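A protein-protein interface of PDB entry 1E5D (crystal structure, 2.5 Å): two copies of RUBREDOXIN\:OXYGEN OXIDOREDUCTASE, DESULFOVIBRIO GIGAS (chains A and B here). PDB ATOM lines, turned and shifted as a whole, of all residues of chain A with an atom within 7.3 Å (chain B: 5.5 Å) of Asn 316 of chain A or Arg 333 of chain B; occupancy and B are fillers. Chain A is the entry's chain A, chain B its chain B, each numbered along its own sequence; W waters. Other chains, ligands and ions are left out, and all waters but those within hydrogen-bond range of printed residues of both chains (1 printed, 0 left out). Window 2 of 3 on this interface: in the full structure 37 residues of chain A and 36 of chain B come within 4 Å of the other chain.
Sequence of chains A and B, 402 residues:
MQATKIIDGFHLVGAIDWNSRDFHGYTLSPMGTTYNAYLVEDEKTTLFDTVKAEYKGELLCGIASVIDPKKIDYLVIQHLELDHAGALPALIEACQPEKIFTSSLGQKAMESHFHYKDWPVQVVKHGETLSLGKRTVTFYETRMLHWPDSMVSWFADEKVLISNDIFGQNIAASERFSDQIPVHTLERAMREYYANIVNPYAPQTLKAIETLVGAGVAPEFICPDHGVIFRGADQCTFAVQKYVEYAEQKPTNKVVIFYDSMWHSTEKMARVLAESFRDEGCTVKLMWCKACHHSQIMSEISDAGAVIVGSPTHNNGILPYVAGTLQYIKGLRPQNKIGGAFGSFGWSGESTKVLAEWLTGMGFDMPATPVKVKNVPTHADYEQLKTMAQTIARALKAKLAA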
ATOM      1  N   THR A 313       1.865   9.426  27.898  1.00  0.00           N
ATOM      2  CA  THR A 313       2.031   9.879  26.515  1.00  0.00           C
ATOM      3  C   THR A 313       1.352  11.225  26.312  1.00  0.00           C
ATOM      4  O   THR A 313       0.158  11.415  26.523  1.00  0.00           O
ATOM      5  CB  THR A 313       1.462   8.857  25.518  1.00  0.00           C
ATOM      6  OG1 THR A 313       2.189   7.636  25.696  1.00  0.00           O
ATOM      7  CG2 THR A 313       1.699   9.342  24.101  1.00  0.00           C
ATOM      8  N   HIS A 314       2.144  12.202  25.879  1.00  0.00           N
ATOM      9  CA  HIS A 314       1.582  13.517  25.609  1.00  0.00           C
ATOM     10  C   HIS A 314       1.807  13.838  24.136  1.00  0.00           C
ATOM     11  O   HIS A 314       2.964  13.953  23.739  1.00  0.00           O
ATOM     12  CB  HIS A 314       2.216  14.578  26.506  1.00  0.00           C
ATOM     13  CG  HIS A 314       1.670  15.956  26.303  1.00  0.00           C
ATOM     14  ND1 HIS A 314       2.390  16.981  25.736  1.00  0.00           N
ATOM     15  CD2 HIS A 314       0.454  16.481  26.589  1.00  0.00           C
ATOM     16  CE1 HIS A 314       1.649  18.071  25.686  1.00  0.00           C
ATOM     17  NE2 HIS A 314       0.460  17.801  26.201  1.00  0.00           N
ATOM     18  N   ASN A 315       0.715  13.960  23.393  1.00  0.00           N
ATOM     19  CA  ASN A 315       0.804  14.242  21.963  1.00  0.00           C
ATOM     20  C   ASN A 315       1.818  13.339  21.270  1.00  0.00           C
ATOM     21  O   ASN A 315       2.797  13.809  20.691  1.00  0.00           O
ATOM     22  CB  ASN A 315       1.143  15.719  21.745  1.00  0.00           C
ATOM     23  CG  ASN A 315       0.046  16.626  22.267  1.00  0.00           C
ATOM     24  OD1 ASN A 315      -1.147  16.336  22.200  1.00  0.00           O
ATOM     25  ND2 ASN A 315       0.469  17.764  22.802  1.00  0.00           N
ATOM     26  N   ASN A 316       1.586  12.032  21.345  1.00  0.00           N
ATOM     27  CA  ASN A 316       2.388  11.057  20.614  1.00  0.00           C
ATOM     28  C   ASN A 316       3.837  11.014  21.065  1.00  0.00           C
ATOM     29  O   ASN A 316       4.685  10.465  20.367  1.00  0.00           O
ATOM     30  CB  ASN A 316       2.309  11.365  19.105  1.00  0.00           C
ATOM     31  CG  ASN A 316       0.844  11.284  18.679  1.00  0.00           C
ATOM     32  OD1 ASN A 316       0.260  12.262  18.227  1.00  0.00           O
ATOM     33  ND2 ASN A 316       0.273  10.095  18.866  1.00  0.00           N
ATOM     34  N   GLY A 317       4.088  11.594  22.234  1.00  0.00           N
ATOM     35  CA  GLY A 317       5.427  11.609  22.789  1.00  0.00           C
ATOM     36  C   GLY A 317       5.400  11.704  24.307  1.00  0.00           C
ATOM     37  O   GLY A 317       4.408  11.361  24.949  1.00  0.00           O
ATOM     38  N   ILE A 318       6.516  12.188  24.841  1.00  0.00           N
ATOM     39  CA  ILE A 318       6.684  12.317  26.281  1.00  0.00           C
ATOM     40  C   ILE A 318       6.582  13.783  26.679  1.00  0.00           C
ATOM     41  O   ILE A 318       6.706  14.659  25.827  1.00  0.00           O
ATOM     42  CB  ILE A 318       8.041  11.755  26.733  1.00  0.00           C
ATOM     43  CG1 ILE A 318       9.227  12.557  26.189  1.00  0.00           C
ATOM     44  CG2 ILE A 318       8.179  10.288  26.367  1.00  0.00           C
ATOM     45  CD1 ILE A 318      10.559  12.183  26.807  1.00  0.00           C
ATOM     46  N   TRP A 347      -4.212   6.185  24.145  1.00  0.00           N
ATOM     47  CA  TRP A 347      -4.507   5.493  22.895  1.00  0.00           C
ATOM     48  C   TRP A 347      -3.238   5.133  22.134  1.00  0.00           C
ATOM     49  O   TRP A 347      -2.976   3.956  21.897  1.00  0.00           O
ATOM     50  CB  TRP A 347      -5.426   6.335  22.016  1.00  0.00           C
ATOM     51  CG  TRP A 347      -5.028   7.747  21.740  1.00  0.00           C
ATOM     52  CD1 TRP A 347      -4.315   8.208  20.667  1.00  0.00           C
ATOM     53  CD2 TRP A 347      -5.322   8.896  22.546  1.00  0.00           C
ATOM     54  NE1 TRP A 347      -4.147   9.569  20.755  1.00  0.00           N
ATOM     55  CE2 TRP A 347      -4.756  10.014  21.902  1.00  0.00           C
ATOM     56  CE3 TRP A 347      -6.009   9.083  23.749  1.00  0.00           C
ATOM     57  CZ2 TRP A 347      -4.854  11.307  22.419  1.00  0.00           C
ATOM     58  CZ3 TRP A 347      -6.106  10.361  24.261  1.00  0.00           C
ATOM     59  CH2 TRP A 347      -5.530  11.452  23.597  1.00  0.00           C
ATOM     60  N   SER A 348      -2.451   6.129  21.744  1.00  0.00           N
ATOM     61  CA  SER A 348      -1.270   5.860  20.923  1.00  0.00           C
ATOM     62  C   SER A 348      -0.202   5.150  21.745  1.00  0.00           C
ATOM     63  O   SER A 348       0.373   4.167  21.267  1.00  0.00           O
ATOM     64  CB  SER A 348      -0.742   7.140  20.290  1.00  0.00           C
ATOM     65  OG  SER A 348      -0.672   8.225  21.182  1.00  0.00           O
ATOM     66  N   GLY A 349       0.064   5.597  22.970  1.00  0.00           N
ATOM     67  CA  GLY A 349       0.946   4.874  23.863  1.00  0.00           C
ATOM     68  C   GLY A 349       2.421   4.897  23.533  1.00  0.00           C
ATOM     69  O   GLY A 349       3.148   3.971  23.917  1.00  0.00           O
ATOM     70  N   GLU A 350       2.938   5.910  22.839  1.00  0.00           N
ATOM     71  CA  GLU A 350       4.348   5.937  22.493  1.00  0.00           C
ATOM     72  C   GLU A 350       5.320   6.145  23.648  1.00  0.00           C
ATOM     73  O   GLU A 350       6.502   5.841  23.456  1.00  0.00           O
ATOM     74  CB  GLU A 350       4.624   7.085  21.491  1.00  0.00           C
ATOM     75  CG  GLU A 350       4.052   6.835  20.110  1.00  0.00           C
ATOM     76  CD  GLU A 350       2.723   7.533  19.902  1.00  0.00           C
ATOM     77  OE1 GLU A 350       1.954   7.630  20.882  1.00  0.00           O
ATOM     78  OE2 GLU A 350       2.473   7.972  18.761  1.00  0.00           O
ATOM     79  N   SER A 351       4.933   6.679  24.794  1.00  0.00           N
ATOM     80  CA  SER A 351       5.905   7.168  25.772  1.00  0.00           C
ATOM     81  C   SER A 351       6.903   6.104  26.200  1.00  0.00           C
ATOM     82  O   SER A 351       8.111   6.353  26.216  1.00  0.00           O
ATOM     83  CB  SER A 351       5.206   7.756  27.005  1.00  0.00           C
ATOM     84  OG  SER A 351       4.400   6.798  27.665  1.00  0.00           O
ATOM     85  N   VAL A 354       9.343   5.380  23.522  1.00  0.00           N
ATOM     86  CA  VAL A 354      10.297   6.471  23.424  1.00  0.00           C
ATOM     87  C   VAL A 354      11.285   6.495  24.582  1.00  0.00           C
ATOM     88  O   VAL A 354      12.490   6.670  24.377  1.00  0.00           O
ATOM     89  CB  VAL A 354       9.578   7.833  23.365  1.00  0.00           C
ATOM     90  CG1 VAL A 354      10.578   8.952  23.586  1.00  0.00           C
ATOM     91  CG2 VAL A 354       8.871   7.996  22.028  1.00  0.00           C
ATOM     92  N   ASN B 199      -4.721  22.004  18.778  1.00  0.00           N
ATOM     93  CA  ASN B 199      -3.971  22.230  17.554  1.00  0.00           C
ATOM     94  C   ASN B 199      -3.605  20.990  16.760  1.00  0.00           C
ATOM     95  O   ASN B 199      -3.804  20.986  15.538  1.00  0.00           O
ATOM     96  CB  ASN B 199      -2.669  22.987  17.880  1.00  0.00           C
ATOM     97  CG  ASN B 199      -2.253  23.857  16.708  1.00  0.00           C
ATOM     98  OD1 ASN B 199      -2.848  24.900  16.439  1.00  0.00           O
ATOM     99  ND2 ASN B 199      -1.214  23.399  16.031  1.00  0.00           N
ATOM    100  N   PRO B 200      -3.064  19.934  17.343  1.00  0.00           N
ATOM    101  CA  PRO B 200      -2.652  18.795  16.505  1.00  0.00           C
ATOM    102  C   PRO B 200      -3.834  18.116  15.815  1.00  0.00           C
ATOM    103  O   PRO B 200      -3.645  17.323  14.894  1.00  0.00           O
ATOM    104  CB  PRO B 200      -1.988  17.836  17.497  1.00  0.00           C
ATOM    105  CG  PRO B 200      -2.535  18.219  18.825  1.00  0.00           C
ATOM    106  CD  PRO B 200      -2.795  19.704  18.768  1.00  0.00           C
ATOM    107  N   TYR B 201      -5.050  18.417  16.250  1.00  0.00           N
ATOM    108  CA  TYR B 201      -6.270  17.938  15.620  1.00  0.00           C
ATOM    109  C   TYR B 201      -6.990  19.075  14.911  1.00  0.00           C
ATOM    110  O   TYR B 201      -8.216  19.190  14.913  1.00  0.00           O
ATOM    111  CB  TYR B 201      -7.178  17.279  16.666  1.00  0.00           C
ATOM    112  CG  TYR B 201      -6.352  16.391  17.578  1.00  0.00           C
ATOM    113  CD1 TYR B 201      -5.843  15.188  17.113  1.00  0.00           C
ATOM    114  CD2 TYR B 201      -6.087  16.782  18.883  1.00  0.00           C
ATOM    115  CE1 TYR B 201      -5.087  14.379  17.936  1.00  0.00           C
ATOM    116  CE2 TYR B 201      -5.329  15.972  19.710  1.00  0.00           C
ATOM    117  CZ  TYR B 201      -4.835  14.777  19.230  1.00  0.00           C
ATOM    118  OH  TYR B 201      -4.079  13.974  20.059  1.00  0.00           O
ATOM    119  N   GLN B 249      -4.486  27.933  10.657  1.00  0.00           N
ATOM    120  CA  GLN B 249      -3.065  28.193  10.886  1.00  0.00           C
ATOM    121  C   GLN B 249      -2.431  28.895   9.703  1.00  0.00           C
ATOM    122  O   GLN B 249      -1.324  28.610   9.239  1.00  0.00           O
ATOM    123  CB  GLN B 249      -2.352  26.867  11.191  1.00  0.00           C
ATOM    124  CG  GLN B 249      -2.841  26.224  12.482  1.00  0.00           C
ATOM    125  CD  GLN B 249      -2.110  24.951  12.827  1.00  0.00           C
ATOM    126  OE1 GLN B 249      -1.026  24.956  13.399  1.00  0.00           O
ATOM    127  NE2 GLN B 249      -2.711  23.818  12.479  1.00  0.00           N
ATOM    128  N   ILE B 329       6.293  21.660  21.155  1.00  0.00           N
ATOM    129  CA  ILE B 329       5.838  22.252  19.914  1.00  0.00           C
ATOM    130  C   ILE B 329       5.566  21.207  18.846  1.00  0.00           C
ATOM    131  O   ILE B 329       4.543  21.232  18.173  1.00  0.00           O
ATOM    132  CB  ILE B 329       6.899  23.242  19.393  1.00  0.00           C
ATOM    133  CG1 ILE B 329       7.060  24.466  20.295  1.00  0.00           C
ATOM    134  CG2 ILE B 329       6.596  23.656  17.969  1.00  0.00           C
ATOM    135  CD1 ILE B 329       8.042  25.472  19.734  1.00  0.00           C
ATOM    136  N   LYS B 330       6.487  20.271  18.673  1.00  0.00           N
ATOM    137  CA  LYS B 330       6.342  19.251  17.639  1.00  0.00           C
ATOM    138  C   LYS B 330       5.063  18.456  17.864  1.00  0.00           C
ATOM    139  O   LYS B 330       4.379  18.127  16.902  1.00  0.00           O
ATOM    140  CB  LYS B 330       7.559  18.339  17.641  1.00  0.00           C
ATOM    141  CG  LYS B 330       7.401  16.962  17.020  1.00  0.00           C
ATOM    142  CD  LYS B 330       8.769  16.297  16.899  1.00  0.00           C
ATOM    143  CE  LYS B 330       8.780  15.169  15.886  1.00  0.00           C
ATOM    144  NZ  LYS B 330       8.998  15.645  14.489  1.00  0.00           N
ATOM    145  N   GLY B 331       4.773  18.160  19.125  1.00  0.00           N
ATOM    146  CA  GLY B 331       3.607  17.396  19.515  1.00  0.00           C
ATOM    147  C   GLY B 331       2.316  18.075  19.104  1.00  0.00           C
ATOM    148  O   GLY B 331       1.326  17.423  18.778  1.00  0.00           O
ATOM    149  N   LEU B 332       2.331  19.404  19.119  1.00  0.00           N
ATOM    150  CA  LEU B 332       1.124  20.145  18.792  1.00  0.00           C
ATOM    151  C   LEU B 332       1.005  20.396  17.298  1.00  0.00           C
ATOM    152  O   LEU B 332       0.003  20.943  16.841  1.00  0.00           O
ATOM    153  CB  LEU B 332       1.138  21.474  19.550  1.00  0.00           C
ATOM    154  CG  LEU B 332       0.860  21.341  21.051  1.00  0.00           C
ATOM    155  CD1 LEU B 332       1.279  22.623  21.749  1.00  0.00           C
ATOM    156  CD2 LEU B 332      -0.601  21.004  21.283  1.00  0.00           C
ATOM    157  N   ARG B 333       2.019  19.994  16.547  1.00  0.00           N
ATOM    158  CA  ARG B 333       2.026  20.028  15.094  1.00  0.00           C
ATOM    159  C   ARG B 333       1.610  21.359  14.493  1.00  0.00           C
ATOM    160  O   ARG B 333       0.601  21.436  13.781  1.00  0.00           O
ATOM    161  CB  ARG B 333       1.085  18.929  14.563  1.00  0.00           C
ATOM    162  CG  ARG B 333       1.430  17.545  15.091  1.00  0.00           C
ATOM    163  CD  ARG B 333       0.795  16.448  14.256  1.00  0.00           C
ATOM    164  NE  ARG B 333       0.313  15.330  15.060  1.00  0.00           N
ATOM    165  CZ  ARG B 333      -0.840  14.696  14.882  1.00  0.00           C
ATOM    166  NH1 ARG B 333      -1.665  15.063  13.908  1.00  0.00           N
ATOM    167  NH2 ARG B 333      -1.175  13.688  15.678  1.00  0.00           N
ATOM    168  N   PRO B 334       2.358  22.428  14.723  1.00  0.00           N
ATOM    169  CA  PRO B 334       2.026  23.694  14.054  1.00  0.00           C
ATOM    170  C   PRO B 334       2.231  23.537  12.547  1.00  0.00           C
ATOM    171  O   PRO B 334       3.200  22.897  12.131  1.00  0.00           O
ATOM    172  CB  PRO B 334       3.047  24.667  14.641  1.00  0.00           C
ATOM    173  CG  PRO B 334       4.207  23.801  15.027  1.00  0.00           C
ATOM    174  CD  PRO B 334       3.559  22.543  15.566  1.00  0.00           C
ATOM    175  N   GLN B 335       1.347  24.104  11.750  1.00  0.00           N
ATOM    176  CA  GLN B 335       1.379  24.049  10.303  1.00  0.00           C
ATOM    177  C   GLN B 335       1.763  25.380   9.668  1.00  0.00           C
ATOM    178  O   GLN B 335       1.627  26.449  10.249  1.00  0.00           O
ATOM    179  CB  GLN B 335      -0.006  23.697   9.731  1.00  0.00           C
ATOM    180  CG  GLN B 335      -0.598  22.384  10.212  1.00  0.00           C
ATOM    181  CD  GLN B 335       0.282  21.211   9.823  1.00  0.00           C
ATOM    182  OE1 GLN B 335       0.897  20.591  10.681  1.00  0.00           O
ATOM    183  NE2 GLN B 335       0.343  20.925   8.529  1.00  0.00           N
HETATM  184  O   HOH W   1       1.477  14.756  17.463  1.00  0.00           O
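The side-chain amide oxygen (OD1) of Asn 316 of chain A is in hydrogen-bond range of the guanidinium group (NH2) of Arg 333 of chain B (3.3 Å).
Asn 316 of chain A touches just one residue of chain B: Arg 333 (3.3 Å). Of the printed residues of chain B, Trp 347 of chain A touches Tyr 201 (3.6 Å). Printed residues of chain A within 4 Å of Tyr 201 of chain B: Trp 347. Lys 330 of chain B touches none of the printed residues of chain A. Printed residues of chain A within 4 Å of Leu 332 of chain B: Asn 315 (3.7 Å). Of chain A, only Asn 316 (3.3 Å) comes within 4 Å of Arg 333 of chain B.
Asn 315 of chain A touches Gly 331 of chain B (CB to O, 3.4 Å). Asn 315 of chain A touches Leu 332 of chain B. Trp 347 of chain A touches Tyr 201 of chain B (CZ2 to OH, 3.6 Å).
Water W1 lies within hydrogen-bond range of NE of Arg 333 of chain B (2.7 Å), OD1 of Asn 316 of chain A (2.9 Å) and O of Gly 331 of chain B (3.0 Å).
Of the 12 printed residues of chain A, 3 touch a printed residue of chain B. Hydrophobic or aromatic side chains of chain A within 4 Å of the printed part of chain B: Trp 347. Hydrophobic or aromatic side chains of chain B that line the printed part of chain A: Tyr 201 and Leu 332.
The side-chain amide nitrogen (ND2) of Asn 199 of chain B sits at hydrogen-bond distance from the backbone carbonyl oxygen (O) of Leu 332 of chain B (2.9 Å). The side-chain hydroxyl of Ser 348 of chain A sits at hydrogen-bond distance from the side-chain amide nitrogen of Asn 316 of chain A (3.1 Å). A ring nitrogen (NE2) of His 314 of chain A sits close to the side-chain amide nitrogen (ND2) of Asn 315 of chain A. The side-chain amide nitrogen of Asn 316 of chain A is in hydrogen-bond range of the side-chain carboxylate of Glu 350 of chain A (3.1 Å). The side-chain amide oxygen (OE1) of Gln 335 of chain B sits close to the backbone carbonyl oxygen (O) of Arg 333 of chain B (3.2 Å). The guanidinium group of Arg 333 of chain B lies within hydrogen-bond range of the backbone carbonyl oxygen of Pro 200 of chain B.
No position is printed for both chains. Of the 4 pairs that touch across the chains among the printed residues, none has its exchanged pair printed and touching as well.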
